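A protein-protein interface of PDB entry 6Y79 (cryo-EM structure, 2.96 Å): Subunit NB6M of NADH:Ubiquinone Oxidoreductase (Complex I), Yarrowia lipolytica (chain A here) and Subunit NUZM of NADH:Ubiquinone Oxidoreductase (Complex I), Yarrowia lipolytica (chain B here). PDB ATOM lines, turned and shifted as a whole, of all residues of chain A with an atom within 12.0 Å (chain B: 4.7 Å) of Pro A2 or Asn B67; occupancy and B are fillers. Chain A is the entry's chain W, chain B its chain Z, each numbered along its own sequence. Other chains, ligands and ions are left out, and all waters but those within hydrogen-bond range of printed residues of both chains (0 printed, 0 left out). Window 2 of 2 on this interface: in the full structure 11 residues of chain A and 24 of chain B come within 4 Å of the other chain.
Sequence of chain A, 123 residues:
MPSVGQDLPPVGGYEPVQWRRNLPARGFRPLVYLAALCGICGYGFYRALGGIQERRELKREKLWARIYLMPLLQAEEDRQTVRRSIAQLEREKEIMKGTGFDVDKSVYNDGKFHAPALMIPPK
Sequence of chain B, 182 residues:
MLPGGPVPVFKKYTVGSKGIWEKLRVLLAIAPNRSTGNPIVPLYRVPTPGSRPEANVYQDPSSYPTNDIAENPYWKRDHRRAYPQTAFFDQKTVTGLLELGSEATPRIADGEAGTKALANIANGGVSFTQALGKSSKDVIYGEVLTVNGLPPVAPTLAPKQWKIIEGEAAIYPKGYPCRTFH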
ATOM      1  N   PRO A   2     -23.889  24.572 -13.765  1.00  0.00           N
ATOM      2  CA  PRO A   2     -23.519  24.225 -15.138  1.00  0.00           C
ATOM      3  C   PRO A   2     -22.082  24.616 -15.453  1.00  0.00           C
ATOM      4  O   PRO A   2     -21.477  25.358 -14.684  1.00  0.00           O
ATOM      5  CB  PRO A   2     -24.503  25.039 -15.971  1.00  0.00           C
ATOM      6  CG  PRO A   2     -24.738  26.259 -15.149  1.00  0.00           C
ATOM      7  CD  PRO A   2     -24.662  25.826 -13.705  1.00  0.00           C
ATOM      8  N   SER A   3     -21.552  24.142 -16.576  1.00  0.00           N
ATOM      9  CA  SER A   3     -20.186  24.427 -16.990  1.00  0.00           C
ATOM     10  C   SER A   3     -20.205  25.304 -18.234  1.00  0.00           C
ATOM     11  O   SER A   3     -20.619  24.851 -19.305  1.00  0.00           O
ATOM     12  CB  SER A   3     -19.422  23.129 -17.261  1.00  0.00           C
ATOM     13  OG  SER A   3     -18.116  23.391 -17.737  1.00  0.00           O
ATOM     14  N   VAL A   4     -19.781  26.569 -18.085  1.00  0.00           N
ATOM     15  CA  VAL A   4     -19.635  27.508 -19.199  1.00  0.00           C
ATOM     16  C   VAL A   4     -18.306  28.246 -19.074  1.00  0.00           C
ATOM     17  O   VAL A   4     -18.018  28.854 -18.039  1.00  0.00           O
ATOM     18  CB  VAL A   4     -20.778  28.547 -19.272  1.00  0.00           C
ATOM     19  CG1 VAL A   4     -20.688  29.316 -20.579  1.00  0.00           C
ATOM     20  CG2 VAL A   4     -22.172  27.934 -19.132  1.00  0.00           C
ATOM     21  N   GLY A   5     -17.496  28.223 -20.130  1.00  0.00           N
ATOM     22  CA  GLY A   5     -16.316  29.063 -20.204  1.00  0.00           C
ATOM     23  C   GLY A   5     -15.049  28.469 -19.639  1.00  0.00           C
ATOM     24  O   GLY A   5     -14.075  29.205 -19.439  1.00  0.00           O
ATOM     25  N   GLN A   6     -15.022  27.171 -19.379  1.00  0.00           N
ATOM     26  CA  GLN A   6     -13.838  26.533 -18.833  1.00  0.00           C
ATOM     27  C   GLN A   6     -12.876  26.126 -19.936  1.00  0.00           C
ATOM     28  O   GLN A   6     -13.219  26.091 -21.118  1.00  0.00           O
ATOM     29  CB  GLN A   6     -14.198  25.284 -18.045  1.00  0.00           C
ATOM     30  CG  GLN A   6     -14.879  25.477 -16.744  1.00  0.00           C
ATOM     31  CD  GLN A   6     -15.109  24.146 -16.100  1.00  0.00           C
ATOM     32  OE1 GLN A   6     -15.239  23.140 -16.786  1.00  0.00           O
ATOM     33  NE2 GLN A   6     -15.111  24.114 -14.787  1.00  0.00           N
ATOM     34  N   ASP A   7     -11.656  25.807 -19.521  1.00  0.00           N
ATOM     35  CA  ASP A   7     -10.705  25.115 -20.373  1.00  0.00           C
ATOM     36  C   ASP A   7     -11.079  23.641 -20.411  1.00  0.00           C
ATOM     37  O   ASP A   7     -11.198  22.994 -19.370  1.00  0.00           O
ATOM     38  CB  ASP A   7      -9.285  25.303 -19.836  1.00  0.00           C
ATOM     39  CG  ASP A   7      -8.207  24.894 -20.820  1.00  0.00           C
ATOM     40  OD1 ASP A   7      -8.517  24.401 -21.928  1.00  0.00           O
ATOM     41  OD2 ASP A   7      -7.026  25.093 -20.481  1.00  0.00           O
ATOM     42  N   LEU A   8     -11.279  23.120 -21.608  1.00  0.00           N
ATOM     43  CA  LEU A   8     -11.664  21.744 -21.870  1.00  0.00           C
ATOM     44  C   LEU A   8     -10.713  21.183 -22.914  1.00  0.00           C
ATOM     45  O   LEU A   8     -10.071  21.943 -23.645  1.00  0.00           O
ATOM     46  CB  LEU A   8     -13.109  21.642 -22.391  1.00  0.00           C
ATOM     47  CG  LEU A   8     -14.328  21.561 -21.473  1.00  0.00           C
ATOM     48  CD1 LEU A   8     -14.219  20.387 -20.532  1.00  0.00           C
ATOM     49  CD2 LEU A   8     -14.550  22.840 -20.730  1.00  0.00           C
ATOM     50  N   ASP B  60     -19.321  29.754 -12.877  1.00  0.00           N
ATOM     51  CA  ASP B  60     -18.744  28.823 -11.909  1.00  0.00           C
ATOM     52  C   ASP B  60     -19.357  27.435 -12.057  1.00  0.00           C
ATOM     53  O   ASP B  60     -20.585  27.306 -12.135  1.00  0.00           O
ATOM     54  CB  ASP B  60     -18.927  29.317 -10.480  1.00  0.00           C
ATOM     55  CG  ASP B  60     -18.207  28.439  -9.472  1.00  0.00           C
ATOM     56  OD1 ASP B  60     -16.963  28.496  -9.418  1.00  0.00           O
ATOM     57  OD2 ASP B  60     -18.875  27.681  -8.738  1.00  0.00           O
ATOM     58  N   PRO B  61     -18.548  26.383 -12.079  1.00  0.00           N
ATOM     59  CA  PRO B  61     -19.068  25.044 -12.353  1.00  0.00           C
ATOM     60  C   PRO B  61     -19.714  24.382 -11.150  1.00  0.00           C
ATOM     61  O   PRO B  61     -19.597  24.826 -10.003  1.00  0.00           O
ATOM     62  CB  PRO B  61     -17.819  24.275 -12.774  1.00  0.00           C
ATOM     63  CG  PRO B  61     -16.738  24.948 -12.023  1.00  0.00           C
ATOM     64  CD  PRO B  61     -17.077  26.394 -12.097  1.00  0.00           C
ATOM     65  N   SER B  62     -20.391  23.276 -11.448  1.00  0.00           N
ATOM     66  CA  SER B  62     -21.337  22.660 -10.530  1.00  0.00           C
ATOM     67  C   SER B  62     -21.632  21.255 -11.028  1.00  0.00           C
ATOM     68  O   SER B  62     -21.520  20.972 -12.224  1.00  0.00           O
ATOM     69  CB  SER B  62     -22.652  23.442 -10.457  1.00  0.00           C
ATOM     70  OG  SER B  62     -22.514  24.796 -10.092  1.00  0.00           O
ATOM     71  N   SER B  63     -22.019  20.382 -10.099  1.00  0.00           N
ATOM     72  CA  SER B  63     -22.619  19.096 -10.422  1.00  0.00           C
ATOM     73  C   SER B  63     -24.112  19.146 -10.132  1.00  0.00           C
ATOM     74  O   SER B  63     -24.574  19.986  -9.361  1.00  0.00           O
ATOM     75  CB  SER B  63     -21.951  17.985  -9.627  1.00  0.00           C
ATOM     76  OG  SER B  63     -20.578  17.877  -9.944  1.00  0.00           O
ATOM     77  N   TYR B  64     -24.866  18.207 -10.729  1.00  0.00           N
ATOM     78  CA  TYR B  64     -26.325  18.336 -10.696  1.00  0.00           C
ATOM     79  C   TYR B  64     -26.957  18.078  -9.328  1.00  0.00           C
ATOM     80  O   TYR B  64     -27.725  18.944  -8.874  1.00  0.00           O
ATOM     81  CB  TYR B  64     -26.992  17.476 -11.772  1.00  0.00           C
ATOM     82  CG  TYR B  64     -28.499  17.508 -11.589  1.00  0.00           C
ATOM     83  CD1 TYR B  64     -29.212  18.687 -11.797  1.00  0.00           C
ATOM     84  CD2 TYR B  64     -29.203  16.381 -11.168  1.00  0.00           C
ATOM     85  CE1 TYR B  64     -30.579  18.739 -11.609  1.00  0.00           C
ATOM     86  CE2 TYR B  64     -30.574  16.426 -10.977  1.00  0.00           C
ATOM     87  CZ  TYR B  64     -31.256  17.606 -11.201  1.00  0.00           C
ATOM     88  OH  TYR B  64     -32.620  17.656 -11.018  1.00  0.00           O
ATOM     89  N   PRO B  65     -26.727  16.957  -8.624  1.00  0.00           N
ATOM     90  CA  PRO B  65     -27.453  16.780  -7.356  1.00  0.00           C
ATOM     91  C   PRO B  65     -26.935  17.647  -6.216  1.00  0.00           C
ATOM     92  O   PRO B  65     -27.377  17.467  -5.077  1.00  0.00           O
ATOM     93  CB  PRO B  65     -27.265  15.285  -7.039  1.00  0.00           C
ATOM     94  CG  PRO B  65     -26.681  14.685  -8.261  1.00  0.00           C
ATOM     95  CD  PRO B  65     -25.872  15.776  -8.855  1.00  0.00           C
ATOM     96  N   THR B  66     -26.018  18.573  -6.477  1.00  0.00           N
ATOM     97  CA  THR B  66     -25.573  19.557  -5.509  1.00  0.00           C
ATOM     98  C   THR B  66     -26.030  20.966  -5.831  1.00  0.00           C
ATOM     99  O   THR B  66     -26.573  21.643  -4.956  1.00  0.00           O
ATOM    100  CB  THR B  66     -24.053  19.543  -5.409  1.00  0.00           C
ATOM    101  OG1 THR B  66     -23.612  18.202  -5.173  1.00  0.00           O
ATOM    102  CG2 THR B  66     -23.631  20.428  -4.271  1.00  0.00           C
ATOM    103  N   ASN B  67     -25.880  21.422  -7.078  1.00  0.00           N
ATOM    104  CA  ASN B  67     -26.379  22.751  -7.412  1.00  0.00           C
ATOM    105  C   ASN B  67     -27.892  22.812  -7.492  1.00  0.00           C
ATOM    106  O   ASN B  67     -28.429  23.907  -7.697  1.00  0.00           O
ATOM    107  CB  ASN B  67     -25.800  23.259  -8.739  1.00  0.00           C
ATOM    108  CG  ASN B  67     -26.283  22.475  -9.984  1.00  0.00           C
ATOM    109  OD1 ASN B  67     -26.947  21.449  -9.910  1.00  0.00           O
ATOM    110  ND2 ASN B  67     -25.944  23.005 -11.151  1.00  0.00           N
ATOM    111  N   ASP B  68     -28.546  21.650  -7.421  1.00  0.00           N
ATOM    112  CA  ASP B  68     -29.987  21.514  -7.524  1.00  0.00           C
ATOM    113  C   ASP B  68     -30.685  22.407  -6.520  1.00  0.00           C
ATOM    114  O   ASP B  68     -30.338  22.434  -5.337  1.00  0.00           O
ATOM    115  CB  ASP B  68     -30.382  20.057  -7.293  1.00  0.00           C
ATOM    116  CG  ASP B  68     -31.757  19.748  -7.815  1.00  0.00           C
ATOM    117  OD1 ASP B  68     -32.363  20.651  -8.411  1.00  0.00           O
ATOM    118  OD2 ASP B  68     -32.231  18.612  -7.620  1.00  0.00           O
ATOM    119  N   ILE B  69     -31.657  23.159  -7.015  1.00  0.00           N
ATOM    120  CA  ILE B  69     -32.187  24.241  -6.211  1.00  0.00           C
ATOM    121  C   ILE B  69     -33.163  23.717  -5.166  1.00  0.00           C
ATOM    122  O   ILE B  69     -33.161  24.184  -4.026  1.00  0.00           O
ATOM    123  CB  ILE B  69     -32.792  25.327  -7.123  1.00  0.00           C
ATOM    124  CG1 ILE B  69     -33.071  26.587  -6.331  1.00  0.00           C
ATOM    125  CG2 ILE B  69     -34.028  24.865  -7.900  1.00  0.00           C
ATOM    126  CD1 ILE B  69     -33.411  27.727  -7.202  1.00  0.00           C
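Among the printed residues, pairs that only touch across the chains: Gln A6 with Pro B61 (3.3 Å), Pro A2 with Pro B61 (3.4 Å), Pro A2 with Asn B67 (3.7 Å) and Pro A2 with Ser B62 (3.7 Å).
Pro A2 touches four residues of chain B.
Of chain A, only Pro A2 comes within 4 Å of Asn B67.
Of chain A, only Pro A2 (3.3 Å) comes within 4 Å of Asp B60.
Of chain A, only Pro A2 (3.4 Å) and Gln A6 (3.3 Å) come within 4 Å of Pro B61.
Ser B62 touches just one residue of chain A: Pro A2 (3.7 Å).
No residue of chain A comes within 4 Å of Tyr B64.
No residue of chain A comes within 4 Å of Pro B65.
No residue of chain A comes within 4 Å of Thr B66.
No residue of chain A comes within 4 Å of Asp B68.
No residue of chain A comes within 4 Å of Ile B69.
Of the printed residues of chain B, Gln A6 touches Pro B61 (3.3 Å).
Asp A7 touches none of the printed residues of chain B.
Leu A8 touches none of the printed residues of chain B.
Of the 10 printed residues of chain B, 4 touch a printed residue of chain A.
Of the 7 printed residues of chain A, 2 touch a printed residue of chain B.
Among the printed residues, no Asp or Glu carboxylate lies within 4 Å of a Lys or Arg side-chain nitrogen of the other chain.
The side-chain hydroxyl of Ser A3 lies within hydrogen-bond range of the side-chain amide oxygen of Gln A6, 3.0 Å away.
The backbone carbonyl oxygen (O) of Ser B63 lies close to the side-chain amide oxygen (OD1) of Asn B67, at 2.8 Å.
The backbone carbonyl oxygen (O) of Tyr B64 lies close to the side-chain amide oxygen (OD1) of Asn B67, 2.8 Å away.
O of Asp B60 lies close to O of Pro A2, 3.3 Å away.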
